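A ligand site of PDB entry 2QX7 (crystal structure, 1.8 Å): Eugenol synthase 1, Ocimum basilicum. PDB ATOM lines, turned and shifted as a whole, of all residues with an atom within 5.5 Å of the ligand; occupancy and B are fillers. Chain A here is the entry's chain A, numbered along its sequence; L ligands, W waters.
Water W7 lies within hydrogen-bond range of O16 of the ligand (2.6 Å), O of Phe 41 (2.9 Å), N of Gly 19 (3.0 Å) and N of Thr 20 (3.1 Å).
Water W12 lies within hydrogen-bond range of an oxygen (O4) of the ligand (2.7 Å), the backbone NH of Ala 88 (2.8 Å) and the side-chain amide oxygen of Gln 91 (2.8 Å).
Water W2 lies within hydrogen-bond range of an oxygen (O1) of the ligand and the backbone NH (N) of Ala 317.
Water W4 lies within hydrogen-bond range of the side-chain carboxylate (OE1) of Glu 66 (2.9 Å) and the backbone NH (N) of Leu 67 (2.9 Å).
NZ of Lys 136 is in hydrogen-bond range of O of Asp 115, at 2.9 Å.
The backbone NH of Ala 155 lies within hydrogen-bond range of the backbone carbonyl oxygen of Gly 117 (3.3 Å).
The backbone NH (N) of Asn 156 lies within hydrogen-bond range of the backbone carbonyl oxygen (O) of Gly 117 (3.0 Å).
OG of Ser 114 sits at hydrogen-bond distance from O of Leu 87.
Merely in contact with the ligand: Gly 18 (3.7 Å), Ala 86 (3.3 Å), Leu 87 (3.3 Å), Ala 88 (3.6 Å), Phe 89 (3.3 Å), Gly 117 (3.6 Å), Cys 157 (3.7 Å) and Phe 162 (3.2 Å).
Hydrophobic or aromatic side chains within 4 Å of the ligand: Tyr 22, Ile 23, Leu 87, Ala 88, Phe 89, Phe 158 and Phe 162.
Within 4 Å of the ligand: Gly 18, Thr 20, Gly 21, Tyr 22, Ile 23, Thr 42, Arg 43, Lys 48, Ala 86, Leu 87, Ala 88, Phe 89, Gln 91, Ser 114, Asp 115, Phe 116, Gly 117, Lys 136, Asn 156, Cys 157, Phe 158 and Phe 162.
Along chain A the residues within 4 Å of the ligand span positions 18 to 162.
The nearest printed residue that does not touch the ligand is Ala 316 (4.2 Å).
The side-chain amino group (NZ) of Lys 136 sits at hydrogen-bond distance from an oxygen (O12) of the ligand (2.9 Å).
The backbone carbonyl oxygen (O) of Asn 156 sits at hydrogen-bond distance from a nitrogen (N7) of the ligand, 2.7 Å away.
The side-chain amino group (NZ) of Lys 48 lies within salt-bridge range of an oxygen (O15) of the ligand, 2.6 Å away.
The backbone NH of Arg 43 lies within hydrogen-bond range of an oxygen (O17) of the ligand, at 3.0 Å.
The side-chain hydroxyl (OG1) of Thr 20 lies within hydrogen-bond range of an oxygen (O5) of the ligand (2.7 Å).
A nitrogen (N7) of the ligand sits at hydrogen-bond distance from the backbone carbonyl oxygen (O) of Phe 116 (3.1 Å).
NE of Arg 43 lies within salt-bridge range of O17 of the ligand, at 2.8 Å.
The backbone NH of Phe 158 sits at hydrogen-bond distance from an oxygen (O14) of the ligand, 2.8 Å away.
O9 of the ligand is in hydrogen-bond range of N of Ile 23 (3.1 Å).
N of Tyr 22 is in hydrogen-bond range of O2 of the ligand (2.8 Å).
An oxygen (O5) of the ligand is in hydrogen-bond range of the backbone NH (N) of Gly 21, at 3.2 Å.
The backbone carbonyl oxygen (O) of Ser 114 lies within hydrogen-bond range of an oxygen (O12) of the ligand (3.4 Å).
An oxygen (O12) of the ligand lies within hydrogen-bond range of the side-chain hydroxyl (OG) of Ser 114.
OG1 of Thr 42 sits at hydrogen-bond distance from O16 of the ligand, at 2.6 Å.
NE2 of Gln 91 lies close to N3 of the ligand, 3.3 Å away.
An oxygen (O12) of the ligand lies within hydrogen-bond range of the backbone carbonyl oxygen (O) of Asp 115.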
ATOM      1  N   GLY A  18      11.921  14.807  24.364  1.00  0.00           N
ATOM      2  CA  GLY A  18      11.149  15.170  23.195  1.00  0.00           C
ATOM      3  C   GLY A  18      12.038  15.821  22.153  1.00  0.00           C
ATOM      4  O   GLY A  18      11.563  16.540  21.277  1.00  0.00           O
ATOM      5  N   GLY A  19      13.337  15.559  22.269  1.00  0.00           N
ATOM      6  CA  GLY A  19      14.315  16.125  21.351  1.00  0.00           C
ATOM      7  C   GLY A  19      14.142  15.829  19.870  1.00  0.00           C
ATOM      8  O   GLY A  19      14.597  16.601  19.031  1.00  0.00           O
ATOM      9  N   THR A  20      13.512  14.698  19.544  1.00  0.00           N
ATOM     10  CA  THR A  20      13.281  14.332  18.148  1.00  0.00           C
ATOM     11  C   THR A  20      12.019  15.019  17.657  1.00  0.00           C
ATOM     12  O   THR A  20      11.617  14.857  16.500  1.00  0.00           O
ATOM     13  CB  THR A  20      13.047  12.816  17.967  1.00  0.00           C
ATOM     14  OG1 THR A  20      11.896  12.430  18.735  1.00  0.00           O
ATOM     15  CG2 THR A  20      14.261  12.008  18.414  1.00  0.00           C
ATOM     16  N   GLY A  21      11.395  15.780  18.549  1.00  0.00           N
ATOM     17  CA  GLY A  21      10.155  16.456  18.229  1.00  0.00           C
ATOM     18  C   GLY A  21      10.175  17.572  17.205  1.00  0.00           C
ATOM     19  O   GLY A  21      11.237  18.031  16.788  1.00  0.00           O
ATOM     20  N   TYR A  22       8.977  18.011  16.817  1.00  0.00           N
ATOM     21  CA  TYR A  22       8.834  19.082  15.833  1.00  0.00           C
ATOM     22  C   TYR A  22       9.605  20.312  16.263  1.00  0.00           C
ATOM     23  O   TYR A  22      10.327  20.906  15.462  1.00  0.00           O
ATOM     24  CB  TYR A  22       7.360  19.446  15.615  1.00  0.00           C
ATOM     25  CG  TYR A  22       7.169  20.519  14.565  1.00  0.00           C
ATOM     26  CD1 TYR A  22       7.354  20.231  13.204  1.00  0.00           C
ATOM     27  CD2 TYR A  22       6.877  21.823  14.933  1.00  0.00           C
ATOM     28  CE1 TYR A  22       7.249  21.251  12.242  1.00  0.00           C
ATOM     29  CE2 TYR A  22       6.771  22.839  13.985  1.00  0.00           C
ATOM     30  CZ  TYR A  22       6.964  22.546  12.646  1.00  0.00           C
ATOM     31  OH  TYR A  22       6.890  23.574  11.727  1.00  0.00           O
ATOM     32  N   ILE A  23       9.468  20.709  17.526  1.00  0.00           N
ATOM     33  CA  ILE A  23      10.212  21.880  18.003  1.00  0.00           C
ATOM     34  C   ILE A  23      11.463  21.418  18.739  1.00  0.00           C
ATOM     35  O   ILE A  23      12.488  22.110  18.756  1.00  0.00           O
ATOM     36  CB  ILE A  23       9.351  22.771  18.937  1.00  0.00           C
ATOM     37  CG1 ILE A  23      10.009  24.145  19.100  1.00  0.00           C
ATOM     38  CG2 ILE A  23       9.168  22.097  20.296  1.00  0.00           C
ATOM     39  CD1 ILE A  23      10.001  24.980  17.812  1.00  0.00           C
ATOM     40  N   GLY A  24      11.375  20.234  19.346  1.00  0.00           N
ATOM     41  CA  GLY A  24      12.501  19.696  20.089  1.00  0.00           C
ATOM     42  C   GLY A  24      13.798  19.567  19.310  1.00  0.00           C
ATOM     43  O   GLY A  24      14.874  19.818  19.851  1.00  0.00           O
ATOM     44  N   PHE A  41      16.875  12.300  25.218  1.00  0.00           N
ATOM     45  CA  PHE A  41      16.161  11.123  25.707  1.00  0.00           C
ATOM     46  C   PHE A  41      15.130  10.796  24.624  1.00  0.00           C
ATOM     47  O   PHE A  41      14.425  11.680  24.137  1.00  0.00           O
ATOM     48  CB  PHE A  41      15.444  11.445  27.021  1.00  0.00           C
ATOM     49  CG  PHE A  41      15.020  10.223  27.813  1.00  0.00           C
ATOM     50  CD1 PHE A  41      15.927   9.538  28.613  1.00  0.00           C
ATOM     51  CD2 PHE A  41      13.699   9.773  27.761  1.00  0.00           C
ATOM     52  CE1 PHE A  41      15.535   8.416  29.360  1.00  0.00           C
ATOM     53  CE2 PHE A  41      13.298   8.657  28.508  1.00  0.00           C
ATOM     54  CZ  PHE A  41      14.215   7.986  29.299  1.00  0.00           C
ATOM     55  N   THR A  42      15.051   9.517  24.252  1.00  0.00           N
ATOM     56  CA  THR A  42      14.126   9.077  23.208  1.00  0.00           C
ATOM     57  C   THR A  42      13.647   7.648  23.492  1.00  0.00           C
ATOM     58  O   THR A  42      14.362   6.863  24.115  1.00  0.00           O
ATOM     59  CB  THR A  42      14.829   9.128  21.822  1.00  0.00           C
ATOM     60  OG1 THR A  42      13.956   8.606  20.809  1.00  0.00           O
ATOM     61  CG2 THR A  42      16.128   8.316  21.853  1.00  0.00           C
ATOM     62  N   ARG A  43      12.433   7.316  23.044  1.00  0.00           N
ATOM     63  CA  ARG A  43      11.887   5.985  23.283  1.00  0.00           C
ATOM     64  C   ARG A  43      12.630   4.896  22.511  1.00  0.00           C
ATOM     65  O   ARG A  43      13.130   5.138  21.414  1.00  0.00           O
ATOM     66  CB  ARG A  43      10.411   5.942  22.882  1.00  0.00           C
ATOM     67  CG  ARG A  43       9.476   6.651  23.842  1.00  0.00           C
ATOM     68  CD  ARG A  43       8.103   6.768  23.210  1.00  0.00           C
ATOM     69  NE  ARG A  43       8.181   7.497  21.952  1.00  0.00           N
ATOM     70  CZ  ARG A  43       7.210   7.539  21.050  1.00  0.00           C
ATOM     71  NH1 ARG A  43       7.369   8.221  19.925  1.00  0.00           N
ATOM     72  NH2 ARG A  43       6.070   6.884  21.260  1.00  0.00           N
ATOM     73  N   SER A  46      11.875   3.638  18.369  1.00  0.00           N
ATOM     74  CA  SER A  46      11.953   4.868  17.596  1.00  0.00           C
ATOM     75  C   SER A  46      11.769   4.682  16.104  1.00  0.00           C
ATOM     76  O   SER A  46      12.069   3.628  15.541  1.00  0.00           O
ATOM     77  CB  SER A  46      13.298   5.560  17.851  1.00  0.00           C
ATOM     78  OG  SER A  46      14.374   4.831  17.289  1.00  0.00           O
ATOM     79  N   LYS A  48      12.866   7.325  14.304  1.00  0.00           N
ATOM     80  CA  LYS A  48      13.728   8.448  13.963  1.00  0.00           C
ATOM     81  C   LYS A  48      15.204   8.075  14.025  1.00  0.00           C
ATOM     82  O   LYS A  48      16.026   8.862  14.500  1.00  0.00           O
ATOM     83  CB  LYS A  48      13.471   9.623  14.915  1.00  0.00           C
ATOM     84  CG  LYS A  48      12.014   9.998  15.121  1.00  0.00           C
ATOM     85  CD  LYS A  48      11.276   8.952  15.948  1.00  0.00           C
ATOM     86  CE  LYS A  48      11.966   8.712  17.283  1.00  0.00           C
ATOM     87  NZ  LYS A  48      11.281   7.656  18.085  1.00  0.00           N
ATOM     88  N   GLU A  66      12.204   4.865  28.546  1.00  0.00           N
ATOM     89  CA  GLU A  66      10.817   5.272  28.726  1.00  0.00           C
ATOM     90  C   GLU A  66      10.747   6.179  29.955  1.00  0.00           C
ATOM     91  O   GLU A  66      11.569   6.060  30.860  1.00  0.00           O
ATOM     92  CB  GLU A  66       9.926   4.056  28.981  1.00  0.00           C
ATOM     93  CG  GLU A  66       9.860   3.052  27.840  1.00  0.00           C
ATOM     94  CD  GLU A  66       8.987   3.533  26.686  1.00  0.00           C
ATOM     95  OE1 GLU A  66       8.138   4.411  26.913  1.00  0.00           O
ATOM     96  OE2 GLU A  66       9.154   3.015  25.560  1.00  0.00           O
ATOM     97  N   LEU A  67       9.754   7.067  29.972  1.00  0.00           N
ATOM     98  CA  LEU A  67       9.585   7.992  31.088  1.00  0.00           C
ATOM     99  C   LEU A  67       9.254   7.263  32.383  1.00  0.00           C
ATOM    100  O   LEU A  67       9.435   7.814  33.472  1.00  0.00           O
ATOM    101  CB  LEU A  67       8.482   8.996  30.758  1.00  0.00           C
ATOM    102  CG  LEU A  67       8.789   9.936  29.571  1.00  0.00           C
ATOM    103  CD1 LEU A  67       7.590  10.831  29.310  1.00  0.00           C
ATOM    104  CD2 LEU A  67      10.012  10.785  29.898  1.00  0.00           C
ATOM    105  N   ALA A  86      10.193  19.111  25.708  1.00  0.00           N
ATOM    106  CA  ALA A  86       9.492  19.526  24.503  1.00  0.00           C
ATOM    107  C   ALA A  86       8.475  18.466  24.146  1.00  0.00           C
ATOM    108  O   ALA A  86       8.208  18.218  22.972  1.00  0.00           O
ATOM    109  CB  ALA A  86      10.488  19.733  23.352  1.00  0.00           C
ATOM    110  N   LEU A  87       7.912  17.814  25.161  1.00  0.00           N
ATOM    111  CA  LEU A  87       6.916  16.762  24.919  1.00  0.00           C
ATOM    112  C   LEU A  87       5.609  17.331  24.371  1.00  0.00           C
ATOM    113  O   LEU A  87       5.304  18.514  24.546  1.00  0.00           O
ATOM    114  CB  LEU A  87       6.659  15.982  26.212  1.00  0.00           C
ATOM    115  CG  LEU A  87       7.866  15.178  26.739  1.00  0.00           C
ATOM    116  CD1 LEU A  87       7.521  14.535  28.068  1.00  0.00           C
ATOM    117  CD2 LEU A  87       8.247  14.116  25.730  1.00  0.00           C
ATOM    118  N   ALA A  88       4.837  16.462  23.721  1.00  0.00           N
ATOM    119  CA  ALA A  88       3.563  16.832  23.114  1.00  0.00           C
ATOM    120  C   ALA A  88       2.409  16.914  24.108  1.00  0.00           C
ATOM    121  O   ALA A  88       2.494  16.413  25.232  1.00  0.00           O
ATOM    122  CB  ALA A  88       3.228  15.839  22.011  1.00  0.00           C
ATOM    123  N   PHE A  89       1.306  17.547  23.693  1.00  0.00           N
ATOM    124  CA  PHE A  89       0.157  17.694  24.564  1.00  0.00           C
ATOM    125  C   PHE A  89      -0.324  16.407  25.243  1.00  0.00           C
ATOM    126  O   PHE A  89      -0.648  16.424  26.428  1.00  0.00           O
ATOM    127  CB  PHE A  89      -1.007  18.338  23.797  1.00  0.00           C
ATOM    128  CG  PHE A  89      -1.193  19.800  24.117  1.00  0.00           C
ATOM    129  CD1 PHE A  89      -1.066  20.769  23.124  1.00  0.00           C
ATOM    130  CD2 PHE A  89      -1.468  20.205  25.420  1.00  0.00           C
ATOM    131  CE1 PHE A  89      -1.225  22.130  23.423  1.00  0.00           C
ATOM    132  CE2 PHE A  89      -1.628  21.563  25.733  1.00  0.00           C
ATOM    133  CZ  PHE A  89      -1.499  22.519  24.722  1.00  0.00           C
ATOM    134  N   GLN A  91       1.285  14.091  26.352  1.00  0.00           N
ATOM    135  CA  GLN A  91       2.247  13.745  27.405  1.00  0.00           C
ATOM    136  C   GLN A  91       2.495  14.842  28.455  1.00  0.00           C
ATOM    137  O   GLN A  91       3.415  14.728  29.258  1.00  0.00           O
ATOM    138  CB  GLN A  91       3.587  13.356  26.774  1.00  0.00           C
ATOM    139  CG  GLN A  91       3.670  11.946  26.203  1.00  0.00           C
ATOM    140  CD  GLN A  91       2.793  11.745  24.989  1.00  0.00           C
ATOM    141  OE1 GLN A  91       2.940  12.424  23.972  1.00  0.00           O
ATOM    142  NE2 GLN A  91       1.868  10.787  25.082  1.00  0.00           N
ATOM    143  N   ILE A  92       1.685  15.893  28.465  1.00  0.00           N
ATOM    144  CA  ILE A  92       1.920  16.974  29.413  1.00  0.00           C
ATOM    145  C   ILE A  92       1.976  16.526  30.878  1.00  0.00           C
ATOM    146  O   ILE A  92       2.905  16.892  31.588  1.00  0.00           O
ATOM    147  CB  ILE A  92       0.866  18.099  29.253  1.00  0.00           C
ATOM    148  CG1 ILE A  92       1.021  18.732  27.865  1.00  0.00           C
ATOM    149  CG2 ILE A  92       1.068  19.181  30.314  1.00  0.00           C
ATOM    150  CD1 ILE A  92       2.386  19.363  27.615  1.00  0.00           C
ATOM    151  N   SER A 114       7.327  21.900  29.043  1.00  0.00           N
ATOM    152  CA  SER A 114       6.870  22.056  27.670  1.00  0.00           C
ATOM    153  C   SER A 114       5.708  23.037  27.575  1.00  0.00           C
ATOM    154  O   SER A 114       4.546  22.656  27.681  1.00  0.00           O
ATOM    155  CB  SER A 114       6.441  20.694  27.095  1.00  0.00           C
ATOM    156  OG  SER A 114       6.176  20.795  25.706  1.00  0.00           O
ATOM    157  N   ASP A 115       6.038  24.316  27.373  1.00  0.00           N
ATOM    158  CA  ASP A 115       5.031  25.350  27.203  1.00  0.00           C
ATOM    159  C   ASP A 115       5.110  25.694  25.718  1.00  0.00           C
ATOM    160  O   ASP A 115       4.365  25.140  24.907  1.00  0.00           O
ATOM    161  CB  ASP A 115       5.350  26.575  28.082  1.00  0.00           C
ATOM    162  CG  ASP A 115       4.971  26.357  29.540  1.00  0.00           C
ATOM    163  OD1 ASP A 115       4.019  25.587  29.786  1.00  0.00           O
ATOM    164  OD2 ASP A 115       5.600  26.952  30.439  1.00  0.00           O
ATOM    165  N   PHE A 116       6.018  26.602  25.368  1.00  0.00           N
ATOM    166  CA  PHE A 116       6.252  26.976  23.979  1.00  0.00           C
ATOM    167  C   PHE A 116       5.051  27.354  23.127  1.00  0.00           C
ATOM    168  O   PHE A 116       4.952  26.981  21.954  1.00  0.00           O
ATOM    169  CB  PHE A 116       7.046  25.852  23.308  1.00  0.00           C
ATOM    170  CG  PHE A 116       8.303  25.489  24.055  1.00  0.00           C
ATOM    171  CD1 PHE A 116       8.436  24.255  24.681  1.00  0.00           C
ATOM    172  CD2 PHE A 116       9.327  26.425  24.191  1.00  0.00           C
ATOM    173  CE1 PHE A 116       9.571  23.943  25.444  1.00  0.00           C
ATOM    174  CE2 PHE A 116      10.464  26.134  24.945  1.00  0.00           C
ATOM    175  CZ  PHE A 116      10.583  24.898  25.576  1.00  0.00           C
ATOM    176  N   GLY A 117       4.144  28.117  23.721  1.00  0.00           N
ATOM    177  CA  GLY A 117       2.967  28.562  22.992  1.00  0.00           C
ATOM    178  C   GLY A 117       2.429  29.834  23.603  1.00  0.00           C
ATOM    179  O   GLY A 117       3.173  30.800  23.817  1.00  0.00           O
ATOM    180  N   VAL A 118       1.136  29.842  23.875  1.00  0.00           N
ATOM    181  CA  VAL A 118       0.486  30.984  24.490  1.00  0.00           C
ATOM    182  C   VAL A 118       0.949  31.082  25.942  1.00  0.00           C
ATOM    183  O   VAL A 118       1.520  30.124  26.471  1.00  0.00           O
ATOM    184  CB  VAL A 118      -1.048  30.825  24.457  1.00  0.00           C
ATOM    185  CG1 VAL A 118      -1.537  30.777  23.014  1.00  0.00           C
ATOM    186  CG2 VAL A 118      -1.439  29.528  25.168  1.00  0.00           C
ATOM    187  N   LYS A 136      -0.791  22.265  31.448  1.00  0.00           N
ATOM    188  CA  LYS A 136       0.512  22.920  31.481  1.00  0.00           C
ATOM    189  C   LYS A 136       0.593  23.781  32.750  1.00  0.00           C
ATOM    190  O   LYS A 136       1.658  23.888  33.372  1.00  0.00           O
ATOM    191  CB  LYS A 136       0.689  23.777  30.226  1.00  0.00           C
ATOM    192  CG  LYS A 136       0.789  22.935  28.958  1.00  0.00           C
ATOM    193  CD  LYS A 136       1.266  23.733  27.768  1.00  0.00           C
ATOM    194  CE  LYS A 136       1.474  22.832  26.560  1.00  0.00           C
ATOM    195  NZ  LYS A 136       1.974  23.593  25.379  1.00  0.00           N
ATOM    196  N   ALA A 155       6.480  30.947  23.515  1.00  0.00           N
ATOM    197  CA  ALA A 155       7.052  31.106  22.180  1.00  0.00           C
ATOM    198  C   ALA A 155       6.123  31.713  21.159  1.00  0.00           C
ATOM    199  O   ALA A 155       6.566  32.136  20.092  1.00  0.00           O
ATOM    200  CB  ALA A 155       7.529  29.741  21.676  1.00  0.00           C
ATOM    201  N   ASN A 156       4.837  31.784  21.491  1.00  0.00           N
ATOM    202  CA  ASN A 156       3.810  32.296  20.579  1.00  0.00           C
ATOM    203  C   ASN A 156       3.655  31.322  19.397  1.00  0.00           C
ATOM    204  O   ASN A 156       3.924  30.128  19.560  1.00  0.00           O
ATOM    205  CB  ASN A 156       4.129  33.727  20.141  1.00  0.00           C
ATOM    206  CG  ASN A 156       3.810  34.752  21.238  1.00  0.00           C
ATOM    207  OD1 ASN A 156       2.801  34.612  21.940  1.00  0.00           O
ATOM    208  ND2 ASN A 156       4.643  35.763  21.380  1.00  0.00           N
ATOM    209  N   CYS A 157       3.229  31.786  18.229  1.00  0.00           N
ATOM    210  CA  CYS A 157       3.004  30.869  17.102  1.00  0.00           C
ATOM    211  C   CYS A 157       4.259  30.355  16.384  1.00  0.00           C
ATOM    212  O   CYS A 157       5.162  31.128  16.073  1.00  0.00           O
ATOM    213  CB  CYS A 157       2.081  31.520  16.071  1.00  0.00           C
ATOM    214  SG  CYS A 157       0.496  32.101  16.706  1.00  0.00           S
ATOM    215  N   PHE A 158       4.307  29.045  16.134  1.00  0.00           N
ATOM    216  CA  PHE A 158       5.419  28.464  15.378  1.00  0.00           C
ATOM    217  C   PHE A 158       5.127  28.937  13.945  1.00  0.00           C
ATOM    218  O   PHE A 158       4.115  28.569  13.355  1.00  0.00           O
ATOM    219  CB  PHE A 158       5.386  26.916  15.432  1.00  0.00           C
ATOM    220  CG  PHE A 158       5.835  26.320  16.755  1.00  0.00           C
ATOM    221  CD1 PHE A 158       6.194  27.118  17.835  1.00  0.00           C
ATOM    222  CD2 PHE A 158       5.879  24.936  16.905  1.00  0.00           C
ATOM    223  CE1 PHE A 158       6.584  26.545  19.051  1.00  0.00           C
ATOM    224  CE2 PHE A 158       6.269  24.348  18.117  1.00  0.00           C
ATOM    225  CZ  PHE A 158       6.620  25.167  19.201  1.00  0.00           C
ATOM    226  N   TYR A 161       4.921  26.368  10.854  1.00  0.00           N
ATOM    227  CA  TYR A 161       3.734  25.586  11.136  1.00  0.00           C
ATOM    228  C   TYR A 161       2.462  26.327  10.716  1.00  0.00           C
ATOM    229  O   TYR A 161       1.631  25.786   9.985  1.00  0.00           O
ATOM    230  CB  TYR A 161       3.662  25.287  12.633  1.00  0.00           C
ATOM    231  CG  TYR A 161       2.560  24.324  13.038  1.00  0.00           C
ATOM    232  CD1 TYR A 161       2.848  22.993  13.324  1.00  0.00           C
ATOM    233  CD2 TYR A 161       1.230  24.748  13.134  1.00  0.00           C
ATOM    234  CE1 TYR A 161       1.847  22.108  13.718  1.00  0.00           C
ATOM    235  CE2 TYR A 161       0.229  23.862  13.529  1.00  0.00           C
ATOM    236  CZ  TYR A 161       0.541  22.548  13.823  1.00  0.00           C
ATOM    237  OH  TYR A 161      -0.428  21.675  14.246  1.00  0.00           O
ATOM    238  N   PHE A 162       2.325  27.572  11.151  1.00  0.00           N
ATOM    239  CA  PHE A 162       1.127  28.311  10.823  1.00  0.00           C
ATOM    240  C   PHE A 162       1.112  29.030   9.498  1.00  0.00           C
ATOM    241  O   PHE A 162       0.042  29.376   8.995  1.00  0.00           O
ATOM    242  CB  PHE A 162       0.743  29.258  11.965  1.00  0.00           C
ATOM    243  CG  PHE A 162       0.090  28.539  13.120  1.00  0.00           C
ATOM    244  CD1 PHE A 162       0.795  28.275  14.289  1.00  0.00           C
ATOM    245  CD2 PHE A 162      -1.214  28.080  13.009  1.00  0.00           C
ATOM    246  CE1 PHE A 162       0.204  27.562  15.329  1.00  0.00           C
ATOM    247  CE2 PHE A 162      -1.822  27.363  14.046  1.00  0.00           C
ATOM    248  CZ  PHE A 162      -1.111  27.106  15.210  1.00  0.00           C
ATOM    249  N   ALA A 316       0.245  18.940  14.786  1.00  0.00           N
ATOM    250  CA  ALA A 316       0.482  18.583  16.173  1.00  0.00           C
ATOM    251  C   ALA A 316      -0.404  17.421  16.597  1.00  0.00           C
ATOM    252  O   ALA A 316      -1.471  17.204  16.014  1.00  0.00           O
ATOM    253  CB  ALA A 316       0.238  19.780  17.089  1.00  0.00           C
ATOM    254  N   ALA A 317       0.043  16.692  17.614  1.00  0.00           N
ATOM    255  CA  ALA A 317      -0.685  15.547  18.138  1.00  0.00           C
ATOM    256  C   ALA A 317      -1.609  15.962  19.284  1.00  0.00           C
ATOM    257  O   ALA A 317      -1.208  16.721  20.162  1.00  0.00           O
ATOM    258  CB  ALA A 317       0.304  14.493  18.631  1.00  0.00           C
HETATM  259  P1  LIG L   1       5.891  16.221  18.930  1.00  0.00           P
HETATM  260  O1  LIG L   1       4.538  15.714  18.617  1.00  0.00           O
HETATM  261  O2  LIG L   1       6.868  16.486  17.850  1.00  0.00           O
HETATM  262  O3  LIG L   1       6.438  15.206  20.031  1.00  0.00           O
HETATM  263  C1  LIG L   1       7.672  15.489  20.713  1.00  0.00           C
HETATM  264  C2  LIG L   1       8.243  14.161  21.100  1.00  0.00           C
HETATM  265  O4  LIG L   1       7.459  13.327  22.097  1.00  0.00           O
HETATM  266  C3  LIG L   1       8.350  13.071  20.044  1.00  0.00           C
HETATM  267  O5  LIG L   1       9.361  13.382  19.127  1.00  0.00           O
HETATM  268  C4  LIG L   1       8.595  11.767  20.802  1.00  0.00           C
HETATM  269  O6  LIG L   1       9.981  11.507  20.945  1.00  0.00           O
HETATM  270  C5  LIG L   1       7.934  11.993  22.152  1.00  0.00           C
HETATM  271  N1  LIG L   1       6.772  11.144  22.400  1.00  0.00           N
HETATM  272  C6  LIG L   1       5.688  10.946  21.540  1.00  0.00           C
HETATM  273  N2  LIG L   1       4.786  10.116  22.013  1.00  0.00           N
HETATM  274  C7  LIG L   1       5.292   9.751  23.225  1.00  0.00           C
HETATM  275  C8  LIG L   1       4.795   8.876  24.238  1.00  0.00           C
HETATM  276  N3  LIG L   1       3.629   8.230  24.087  1.00  0.00           N
HETATM  277  N4  LIG L   1       5.561   8.720  25.362  1.00  0.00           N
HETATM  278  C9  LIG L   1       6.750   9.382  25.499  1.00  0.00           C
HETATM  279  N5  LIG L   1       7.308  10.238  24.599  1.00  0.00           N
HETATM  280  C10 LIG L   1       6.525  10.368  23.482  1.00  0.00           C
HETATM  281  O7  LIG L   1       5.694  17.538  19.867  1.00  0.00           O
HETATM  282  P2  LIG L   1       5.588  19.023  19.292  1.00  0.00           P
HETATM  283  O8  LIG L   1       4.606  19.093  18.175  1.00  0.00           O
HETATM  284  O9  LIG L   1       6.980  19.448  18.988  1.00  0.00           O
HETATM  285  O10 LIG L   1       5.087  19.881  20.535  1.00  0.00           O
HETATM  286  C11 LIG L   1       5.930  20.143  21.663  1.00  0.00           C
HETATM  287  C12 LIG L   1       5.462  21.389  22.366  1.00  0.00           C
HETATM  288  O11 LIG L   1       5.327  22.471  21.386  1.00  0.00           O
HETATM  289  C13 LIG L   1       4.108  21.203  23.111  1.00  0.00           C
HETATM  290  O12 LIG L   1       4.129  21.850  24.369  1.00  0.00           O
HETATM  291  C14 LIG L   1       3.172  21.799  22.108  1.00  0.00           C
HETATM  292  O13 LIG L   1       1.968  22.193  22.737  1.00  0.00           O
HETATM  293  C15 LIG L   1       3.961  22.931  21.501  1.00  0.00           C
HETATM  294  N6  LIG L   1       3.398  23.373  20.205  1.00  0.00           N
HETATM  295  C16 LIG L   1       3.267  24.738  20.024  1.00  0.00           C
HETATM  296  C17 LIG L   1       2.927  25.259  18.779  1.00  0.00           C
HETATM  297  C18 LIG L   1       2.887  26.742  18.515  1.00  0.00           C
HETATM  298  O14 LIG L   1       2.621  27.155  17.387  1.00  0.00           O
HETATM  299  N7  LIG L   1       3.194  27.572  19.529  1.00  0.00           N
HETATM  300  C19 LIG L   1       2.637  24.350  17.704  1.00  0.00           C
HETATM  301  C20 LIG L   1       2.761  22.975  17.904  1.00  0.00           C
HETATM  302  C21 LIG L   1       3.164  22.476  19.141  1.00  0.00           C
HETATM  303  P3  LIG L   1      10.650  10.040  20.767  1.00  0.00           P
HETATM  304  O15 LIG L   1      10.008   9.400  19.560  1.00  0.00           O
HETATM  305  O16 LIG L   1      12.101  10.403  20.632  1.00  0.00           O
HETATM  306  O17 LIG L   1      10.354   9.292  22.047  1.00  0.00           O
HETATM  307  O   HOH W   1       9.122  18.702  20.098  1.00  0.00           O
HETATM  308  O   HOH W   2       2.468  17.466  18.817  1.00  0.00           O
HETATM  309  O   HOH W   3       4.017  13.131  19.514  1.00  0.00           O
HETATM  310  O   HOH W   4       8.441   7.250  27.357  1.00  0.00           O
HETATM  311  O   HOH W   5       3.858  19.959  15.787  1.00  0.00           O
HETATM  312  O   HOH W   6       0.558  20.991  20.501  1.00  0.00           O
HETATM  313  O   HOH W   7      13.008  12.594  21.776  1.00  0.00           O
HETATM  314  O   HOH W   8       3.675  15.044  16.054  1.00  0.00           O
HETATM  315  O   HOH W   9      10.285  10.196  24.467  1.00  0.00           O
HETATM  316  O   HOH W  10       7.294  14.687  15.841  1.00  0.00           O
HETATM  317  O   HOH W  11       8.709  10.424  17.500  1.00  0.00           O
HETATM  318  O   HOH W  12       5.396  13.739  23.732  1.00  0.00           O
